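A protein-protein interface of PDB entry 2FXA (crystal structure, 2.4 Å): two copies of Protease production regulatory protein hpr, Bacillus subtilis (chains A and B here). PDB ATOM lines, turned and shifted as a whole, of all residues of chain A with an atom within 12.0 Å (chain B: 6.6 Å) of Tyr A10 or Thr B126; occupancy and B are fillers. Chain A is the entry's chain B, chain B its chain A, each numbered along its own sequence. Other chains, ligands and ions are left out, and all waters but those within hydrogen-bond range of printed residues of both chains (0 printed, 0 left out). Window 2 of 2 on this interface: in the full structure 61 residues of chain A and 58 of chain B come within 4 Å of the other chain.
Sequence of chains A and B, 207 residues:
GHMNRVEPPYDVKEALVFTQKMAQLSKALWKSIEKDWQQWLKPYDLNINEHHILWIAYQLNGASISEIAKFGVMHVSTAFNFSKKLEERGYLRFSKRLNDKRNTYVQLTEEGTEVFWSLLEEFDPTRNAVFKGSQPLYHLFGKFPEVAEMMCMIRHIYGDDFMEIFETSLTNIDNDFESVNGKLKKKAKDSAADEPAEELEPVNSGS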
ATOM      1  N   TYR A  10     -19.070  24.563 -18.383  1.00  0.00           N
ATOM      2  CA  TYR A  10     -19.130  24.776 -19.871  1.00  0.00           C
ATOM      3  C   TYR A  10     -17.864  25.502 -20.356  1.00  0.00           C
ATOM      4  O   TYR A  10     -17.273  26.308 -19.628  1.00  0.00           O
ATOM      5  CB  TYR A  10     -20.421  25.542 -20.305  1.00  0.00           C
ATOM      6  CG  TYR A  10     -20.508  26.946 -19.725  1.00  0.00           C
ATOM      7  CD1 TYR A  10     -19.703  27.979 -20.232  1.00  0.00           C
ATOM      8  CD2 TYR A  10     -21.360  27.239 -18.657  1.00  0.00           C
ATOM      9  CE1 TYR A  10     -19.726  29.268 -19.690  1.00  0.00           C
ATOM     10  CE2 TYR A  10     -21.411  28.538 -18.108  1.00  0.00           C
ATOM     11  CZ  TYR A  10     -20.583  29.551 -18.638  1.00  0.00           C
ATOM     12  OH  TYR A  10     -20.603  30.844 -18.136  1.00  0.00           O
ATOM     13  N   ASP A  11     -17.462  25.190 -21.584  1.00  0.00           N
ATOM     14  CA  ASP A  11     -16.489  25.958 -22.318  1.00  0.00           C
ATOM     15  C   ASP A  11     -17.166  27.159 -23.014  1.00  0.00           C
ATOM     16  O   ASP A  11     -18.034  26.972 -23.876  1.00  0.00           O
ATOM     17  CB  ASP A  11     -15.856  25.039 -23.335  1.00  0.00           C
ATOM     18  CG  ASP A  11     -14.953  25.761 -24.294  1.00  0.00           C
ATOM     19  OD1 ASP A  11     -14.455  26.878 -23.972  1.00  0.00           O
ATOM     20  OD2 ASP A  11     -14.726  25.183 -25.380  1.00  0.00           O
ATOM     21  N   VAL A  12     -16.765  28.378 -22.643  1.00  0.00           N
ATOM     22  CA  VAL A  12     -17.415  29.616 -23.102  1.00  0.00           C
ATOM     23  C   VAL A  12     -17.326  29.788 -24.623  1.00  0.00           C
ATOM     24  O   VAL A  12     -18.236  30.318 -25.228  1.00  0.00           O
ATOM     25  CB  VAL A  12     -16.900  30.879 -22.349  1.00  0.00           C
ATOM     26  CG1 VAL A  12     -15.472  31.262 -22.786  1.00  0.00           C
ATOM     27  CG2 VAL A  12     -17.865  32.058 -22.512  1.00  0.00           C
ATOM     28  N   LYS A  13     -16.241  29.310 -25.227  1.00  0.00           N
ATOM     29  CA  LYS A  13     -16.136  29.244 -26.680  1.00  0.00           C
ATOM     30  C   LYS A  13     -17.107  28.225 -27.318  1.00  0.00           C
ATOM     31  O   LYS A  13     -17.652  28.497 -28.365  1.00  0.00           O
ATOM     32  CB  LYS A  13     -14.696  28.964 -27.124  1.00  0.00           C
ATOM     33  CG  LYS A  13     -13.909  30.219 -27.468  1.00  0.00           C
ATOM     34  CD  LYS A  13     -12.409  29.938 -27.737  1.00  0.00           C
ATOM     35  CE  LYS A  13     -12.200  29.062 -28.997  1.00  0.00           C
ATOM     36  NZ  LYS A  13     -10.723  28.833 -29.337  1.00  0.00           N
ATOM     37  N   GLU A  14     -17.285  27.056 -26.703  1.00  0.00           N
ATOM     38  CA  GLU A  14     -18.285  26.088 -27.133  1.00  0.00           C
ATOM     39  C   GLU A  14     -19.689  26.706 -26.958  1.00  0.00           C
ATOM     40  O   GLU A  14     -20.561  26.571 -27.828  1.00  0.00           O
ATOM     41  CB  GLU A  14     -18.139  24.763 -26.343  1.00  0.00           C
ATOM     42  CG  GLU A  14     -18.719  23.504 -27.047  1.00  0.00           C
ATOM     43  CD  GLU A  14     -19.009  22.256 -26.109  1.00  0.00           C
ATOM     44  OE1 GLU A  14     -19.762  21.335 -26.580  1.00  0.00           O
ATOM     45  OE2 GLU A  14     -18.512  22.183 -24.938  1.00  0.00           O
ATOM     46  N   ALA A  15     -19.898  27.425 -25.859  1.00  0.00           N
ATOM     47  CA  ALA A  15     -21.204  28.030 -25.602  1.00  0.00           C
ATOM     48  C   ALA A  15     -21.560  29.105 -26.652  1.00  0.00           C
ATOM     49  O   ALA A  15     -22.675  29.152 -27.147  1.00  0.00           O
ATOM     50  CB  ALA A  15     -21.246  28.584 -24.210  1.00  0.00           C
ATOM     51  N   LEU A  16     -20.594  29.955 -26.981  1.00  0.00           N
ATOM     52  CA  LEU A  16     -20.718  30.935 -28.050  1.00  0.00           C
ATOM     53  C   LEU A  16     -21.014  30.316 -29.448  1.00  0.00           C
ATOM     54  O   LEU A  16     -21.947  30.743 -30.141  1.00  0.00           O
ATOM     55  CB  LEU A  16     -19.470  31.832 -28.103  1.00  0.00           C
ATOM     56  CG  LEU A  16     -19.542  32.907 -29.204  1.00  0.00           C
ATOM     57  CD1 LEU A  16     -20.549  34.071 -28.878  1.00  0.00           C
ATOM     58  CD2 LEU A  16     -18.173  33.441 -29.542  1.00  0.00           C
ATOM     59  N   VAL A  17     -20.220  29.333 -29.863  1.00  0.00           N
ATOM     60  CA  VAL A  17     -20.472  28.658 -31.131  1.00  0.00           C
ATOM     61  C   VAL A  17     -21.907  28.150 -31.195  1.00  0.00           C
ATOM     62  O   VAL A  17     -22.611  28.331 -32.207  1.00  0.00           O
ATOM     63  CB  VAL A  17     -19.501  27.473 -31.349  1.00  0.00           C
ATOM     64  CG1 VAL A  17     -19.976  26.544 -32.476  1.00  0.00           C
ATOM     65  CG2 VAL A  17     -18.074  27.989 -31.636  1.00  0.00           C
ATOM     66  N   PHE A  18     -22.332  27.506 -30.114  1.00  0.00           N
ATOM     67  CA  PHE A  18     -23.669  26.974 -30.029  1.00  0.00           C
ATOM     68  C   PHE A  18     -24.766  28.075 -30.137  1.00  0.00           C
ATOM     69  O   PHE A  18     -25.632  28.012 -31.006  1.00  0.00           O
ATOM     70  CB  PHE A  18     -23.866  26.094 -28.784  1.00  0.00           C
ATOM     71  CG  PHE A  18     -25.274  25.583 -28.654  1.00  0.00           C
ATOM     72  CD1 PHE A  18     -25.772  24.658 -29.570  1.00  0.00           C
ATOM     73  CD2 PHE A  18     -26.119  26.057 -27.657  1.00  0.00           C
ATOM     74  CE1 PHE A  18     -27.077  24.189 -29.484  1.00  0.00           C
ATOM     75  CE2 PHE A  18     -27.421  25.580 -27.541  1.00  0.00           C
ATOM     76  CZ  PHE A  18     -27.915  24.654 -28.456  1.00  0.00           C
ATOM     77  N   THR A  19     -24.702  29.081 -29.282  1.00  0.00           N
ATOM     78  CA  THR A  19     -25.730  30.114 -29.255  1.00  0.00           C
ATOM     79  C   THR A  19     -25.764  30.917 -30.588  1.00  0.00           C
ATOM     80  O   THR A  19     -26.827  31.343 -31.060  1.00  0.00           O
ATOM     81  CB  THR A  19     -25.540  31.080 -28.056  1.00  0.00           C
ATOM     82  OG1 THR A  19     -24.265  31.685 -28.174  1.00  0.00           O
ATOM     83  CG2 THR A  19     -25.565  30.347 -26.700  1.00  0.00           C
ATOM     84  N   GLN A  20     -24.615  31.102 -31.209  1.00  0.00           N
ATOM     85  CA  GLN A  20     -24.631  31.776 -32.486  1.00  0.00           C
ATOM     86  C   GLN A  20     -25.138  30.886 -33.627  1.00  0.00           C
ATOM     87  O   GLN A  20     -25.798  31.357 -34.551  1.00  0.00           O
ATOM     88  CB  GLN A  20     -23.294  32.465 -32.765  1.00  0.00           C
ATOM     89  CG  GLN A  20     -22.185  31.554 -33.069  1.00  0.00           C
ATOM     90  CD  GLN A  20     -21.533  31.964 -34.379  1.00  0.00           C
ATOM     91  OE1 GLN A  20     -20.541  32.746 -34.380  1.00  0.00           O
ATOM     92  NE2 GLN A  20     -22.123  31.498 -35.517  1.00  0.00           N
ATOM     93  N   HIS A 156     -38.413  23.568 -22.280  1.00  0.00           N
ATOM     94  CA  HIS A 156     -37.655  24.091 -21.145  1.00  0.00           C
ATOM     95  C   HIS A 156     -37.681  25.609 -21.000  1.00  0.00           C
ATOM     96  O   HIS A 156     -37.692  26.101 -19.909  1.00  0.00           O
ATOM     97  CB  HIS A 156     -36.254  23.509 -21.097  1.00  0.00           C
ATOM     98  CG  HIS A 156     -36.237  22.072 -20.659  1.00  0.00           C
ATOM     99  ND1 HIS A 156     -36.085  21.695 -19.338  1.00  0.00           N
ATOM    100  CD2 HIS A 156     -36.436  20.924 -21.354  1.00  0.00           C
ATOM    101  CE1 HIS A 156     -36.153  20.378 -19.247  1.00  0.00           C
ATOM    102  NE2 HIS A 156     -36.368  19.889 -20.457  1.00  0.00           N
ATOM    103  N   ILE A 157     -37.753  26.346 -22.097  1.00  0.00           N
ATOM    104  CA  ILE A 157     -37.835  27.797 -22.044  1.00  0.00           C
ATOM    105  C   ILE A 157     -39.286  28.250 -21.733  1.00  0.00           C
ATOM    106  O   ILE A 157     -39.528  29.092 -20.877  1.00  0.00           O
ATOM    107  CB  ILE A 157     -37.371  28.407 -23.411  1.00  0.00           C
ATOM    108  CG1 ILE A 157     -35.906  28.047 -23.695  1.00  0.00           C
ATOM    109  CG2 ILE A 157     -37.623  29.926 -23.443  1.00  0.00           C
ATOM    110  CD1 ILE A 157     -35.527  28.190 -25.170  1.00  0.00           C
ATOM    111  N   ASP B 124     -22.350  36.294 -22.011  1.00  0.00           N
ATOM    112  CA  ASP B 124     -22.550  35.523 -20.796  1.00  0.00           C
ATOM    113  C   ASP B 124     -23.648  34.513 -21.102  1.00  0.00           C
ATOM    114  O   ASP B 124     -24.820  34.864 -21.136  1.00  0.00           O
ATOM    115  CB  ASP B 124     -22.985  36.476 -19.673  1.00  0.00           C
ATOM    116  CG  ASP B 124     -23.351  35.763 -18.358  1.00  0.00           C
ATOM    117  OD1 ASP B 124     -23.204  34.507 -18.194  1.00  0.00           O
ATOM    118  OD2 ASP B 124     -23.784  36.503 -17.446  1.00  0.00           O
ATOM    119  N   PRO B 125     -23.271  33.260 -21.365  1.00  0.00           N
ATOM    120  CA  PRO B 125     -24.246  32.216 -21.685  1.00  0.00           C
ATOM    121  C   PRO B 125     -25.297  31.907 -20.590  1.00  0.00           C
ATOM    122  O   PRO B 125     -26.382  31.444 -20.913  1.00  0.00           O
ATOM    123  CB  PRO B 125     -23.361  30.988 -21.939  1.00  0.00           C
ATOM    124  CG  PRO B 125     -22.086  31.273 -21.277  1.00  0.00           C
ATOM    125  CD  PRO B 125     -21.893  32.736 -21.405  1.00  0.00           C
ATOM    126  N   THR B 126     -24.997  32.151 -19.323  1.00  0.00           N
ATOM    127  CA  THR B 126     -25.980  31.903 -18.255  1.00  0.00           C
ATOM    128  C   THR B 126     -27.179  32.871 -18.337  1.00  0.00           C
ATOM    129  O   THR B 126     -28.195  32.665 -17.680  1.00  0.00           O
ATOM    130  CB  THR B 126     -25.362  31.975 -16.855  1.00  0.00           C
ATOM    131  OG1 THR B 126     -25.026  33.332 -16.550  1.00  0.00           O
ATOM    132  CG2 THR B 126     -24.110  31.108 -16.762  1.00  0.00           C
ATOM    133  N   ARG B 127     -27.066  33.900 -19.168  1.00  0.00           N
ATOM    134  CA  ARG B 127     -28.170  34.789 -19.421  1.00  0.00           C
ATOM    135  C   ARG B 127     -28.871  34.521 -20.717  1.00  0.00           C
ATOM    136  O   ARG B 127     -29.614  35.366 -21.210  1.00  0.00           O
ATOM    137  CB  ARG B 127     -27.654  36.209 -19.467  1.00  0.00           C
ATOM    138  CG  ARG B 127     -27.175  36.675 -18.079  1.00  0.00           C
ATOM    139  CD  ARG B 127     -26.927  38.120 -18.198  1.00  0.00           C
ATOM    140  NE  ARG B 127     -26.182  38.651 -17.074  1.00  0.00           N
ATOM    141  CZ  ARG B 127     -25.827  39.921 -17.025  1.00  0.00           C
ATOM    142  NH1 ARG B 127     -25.147  40.374 -15.990  1.00  0.00           N
ATOM    143  NH2 ARG B 127     -26.158  40.716 -18.046  1.00  0.00           N
ATOM    144  N   ASN B 128     -28.589  33.388 -21.334  1.00  0.00           N
ATOM    145  CA  ASN B 128     -29.184  33.090 -22.597  1.00  0.00           C
ATOM    146  C   ASN B 128     -30.145  31.927 -22.377  1.00  0.00           C
ATOM    147  O   ASN B 128     -29.761  30.882 -21.847  1.00  0.00           O
ATOM    148  CB  ASN B 128     -28.065  32.772 -23.577  1.00  0.00           C
ATOM    149  CG  ASN B 128     -28.580  32.403 -24.933  1.00  0.00           C
ATOM    150  OD1 ASN B 128     -29.048  31.288 -25.156  1.00  0.00           O
ATOM    151  ND2 ASN B 128     -28.521  33.345 -25.851  1.00  0.00           N
ATOM    152  N   ALA B 129     -31.411  32.136 -22.736  1.00  0.00           N
ATOM    153  CA  ALA B 129     -32.481  31.150 -22.454  1.00  0.00           C
ATOM    154  C   ALA B 129     -32.314  29.838 -23.243  1.00  0.00           C
ATOM    155  O   ALA B 129     -32.533  28.731 -22.717  1.00  0.00           O
ATOM    156  CB  ALA B 129     -33.843  31.757 -22.694  1.00  0.00           C
ATOM    157  N   PHE B 131     -29.342  28.660 -24.442  1.00  0.00           N
ATOM    158  CA  PHE B 131     -28.254  28.001 -23.755  1.00  0.00           C
ATOM    159  C   PHE B 131     -28.806  27.262 -22.520  1.00  0.00           C
ATOM    160  O   PHE B 131     -28.482  26.096 -22.315  1.00  0.00           O
ATOM    161  CB  PHE B 131     -27.108  28.977 -23.385  1.00  0.00           C
ATOM    162  CG  PHE B 131     -26.041  28.354 -22.474  1.00  0.00           C
ATOM    163  CD1 PHE B 131     -24.913  27.721 -23.012  1.00  0.00           C
ATOM    164  CD2 PHE B 131     -26.191  28.363 -21.085  1.00  0.00           C
ATOM    165  CE1 PHE B 131     -23.935  27.142 -22.167  1.00  0.00           C
ATOM    166  CE2 PHE B 131     -25.228  27.745 -20.216  1.00  0.00           C
ATOM    167  CZ  PHE B 131     -24.115  27.146 -20.765  1.00  0.00           C
ATOM    168  N   LYS B 132     -29.622  27.915 -21.692  1.00  0.00           N
ATOM    169  CA  LYS B 132     -30.071  27.224 -20.444  1.00  0.00           C
ATOM    170  C   LYS B 132     -31.087  26.164 -20.768  1.00  0.00           C
ATOM    171  O   LYS B 132     -31.060  25.114 -20.168  1.00  0.00           O
ATOM    172  CB  LYS B 132     -30.658  28.167 -19.386  1.00  0.00           C
ATOM    173  CG  LYS B 132     -29.814  29.391 -19.088  1.00  0.00           C
ATOM    174  CD  LYS B 132     -30.231  30.073 -17.795  1.00  0.00           C
ATOM    175  CE  LYS B 132     -31.513  30.847 -17.961  1.00  0.00           C
ATOM    176  NZ  LYS B 132     -31.219  32.223 -18.350  1.00  0.00           N
ATOM    177  N   GLN B 135     -29.500  22.704 -21.537  1.00  0.00           N
ATOM    178  CA  GLN B 135     -28.630  22.006 -20.580  1.00  0.00           C
ATOM    179  C   GLN B 135     -28.984  20.540 -20.308  1.00  0.00           C
ATOM    180  O   GLN B 135     -28.083  19.694 -20.223  1.00  0.00           O
ATOM    181  CB  GLN B 135     -28.520  22.763 -19.243  1.00  0.00           C
ATOM    182  CG  GLN B 135     -27.725  24.069 -19.303  1.00  0.00           C
ATOM    183  CD  GLN B 135     -26.402  23.950 -20.050  1.00  0.00           C
ATOM    184  OE1 GLN B 135     -26.225  24.533 -21.137  1.00  0.00           O
ATOM    185  NE2 GLN B 135     -25.475  23.202 -19.488  1.00  0.00           N
ATOM    186  N   TYR B 138     -27.572  18.681 -23.126  1.00  0.00           N
ATOM    187  CA  TYR B 138     -26.125  18.672 -22.928  1.00  0.00           C
ATOM    188  C   TYR B 138     -25.683  17.658 -21.883  1.00  0.00           C
ATOM    189  O   TYR B 138     -24.739  16.876 -22.120  1.00  0.00           O
ATOM    190  CB  TYR B 138     -25.599  20.071 -22.560  1.00  0.00           C
ATOM    191  CG  TYR B 138     -24.086  20.153 -22.594  1.00  0.00           C
ATOM    192  CD1 TYR B 138     -23.427  20.644 -23.706  1.00  0.00           C
ATOM    193  CD2 TYR B 138     -23.323  19.728 -21.525  1.00  0.00           C
ATOM    194  CE1 TYR B 138     -22.036  20.710 -23.754  1.00  0.00           C
ATOM    195  CE2 TYR B 138     -21.931  19.785 -21.562  1.00  0.00           C
ATOM    196  CZ  TYR B 138     -21.307  20.275 -22.675  1.00  0.00           C
ATOM    197  OH  TYR B 138     -19.949  20.325 -22.712  1.00  0.00           O
ATOM    198  N   PHE B 144     -23.600  19.835 -27.044  1.00  0.00           N
ATOM    199  CA  PHE B 144     -24.779  20.609 -27.417  1.00  0.00           C
ATOM    200  C   PHE B 144     -25.529  19.879 -28.511  1.00  0.00           C
ATOM    201  O   PHE B 144     -24.923  19.140 -29.285  1.00  0.00           O
ATOM    202  CB  PHE B 144     -24.400  22.004 -27.867  1.00  0.00           C
ATOM    203  CG  PHE B 144     -23.897  22.870 -26.762  1.00  0.00           C
ATOM    204  CD1 PHE B 144     -24.780  23.445 -25.851  1.00  0.00           C
ATOM    205  CD2 PHE B 144     -22.536  23.103 -26.615  1.00  0.00           C
ATOM    206  CE1 PHE B 144     -24.304  24.252 -24.818  1.00  0.00           C
ATOM    207  CE2 PHE B 144     -22.059  23.907 -25.593  1.00  0.00           C
ATOM    208  CZ  PHE B 144     -22.951  24.486 -24.701  1.00  0.00           C
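Tyr A10 touches just these residues of chain B: Pro B125 (3.5 Å), Thr B126 (3.8 Å) and Phe B131 (3.5 Å). Of the printed residues of chain B, Glu A14 touches Tyr B138 (3.2 Å) and Phe B144 (3.3 Å). No residue of chain A comes within 4 Å of Asp B124. Of chain A, only Tyr A10 and Ala A15 come within 4 Å of Pro B125. Asn B128 touches one residue of chain A. Of the printed residues of chain A, Ala B129 touches Ile A157 (3.6 Å). Of chain A, only Tyr A10 (3.5 Å), Ala A15 (3.7 Å) and Thr A19 (3.9 Å) come within 4 Å of Phe B131. Of the printed residues of chain A, Tyr B138 touches Glu A14. The nearest residue of chain A that does not touch Thr B126 is Ala A15 (7.1 Å).
OD1 of Asp B124 sits at hydrogen-bond distance from OG1 of Thr B126. NZ of Lys B132 is in hydrogen-bond range of O of Thr B126, at 3.1 Å. OD1 of Asn B128 is in hydrogen-bond range of N of Phe B131 (2.7 Å). The backbone NH (N) of Glu A14 is in hydrogen-bond range of the side-chain carboxylate (OD2) of Asp A11, at 3.4 Å. O of Ala A15 sits close to OG1 of Thr A19 (3.2 Å). O of Leu A16 is in hydrogen-bond range of OG1 of Thr A19 (3.2 Å).
OE2 of Glu A14 lies within hydrogen-bond range of OH of Tyr B138, at 3.2 Å.
Hydrophobic or aromatic side chains of chain B that line the printed part of chain A: Pro B125, Phe B131, Tyr B138 and Phe B144. Hydrophobic or aromatic side chains of chain A that line the printed part of chain B: Tyr A10, Ala A15, Phe A18 and Ile A157. Along chain A the printed residues that touch a printed residue of chain B span positions 10 to 157.
No position is printed for both chains.
Among the printed residues, pairs that only touch across the chains: Tyr A10 with Pro B125, Tyr A10 with Thr B126, Tyr A10 with Phe B131, Glu A14 with Phe B144, Ala A15 with Pro B125, Ala A15 with Phe B131, Phe A18 with Phe B144, Thr A19 with Asn B128, Thr A19 with Phe B131 and Ile A157 with Ala B129.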
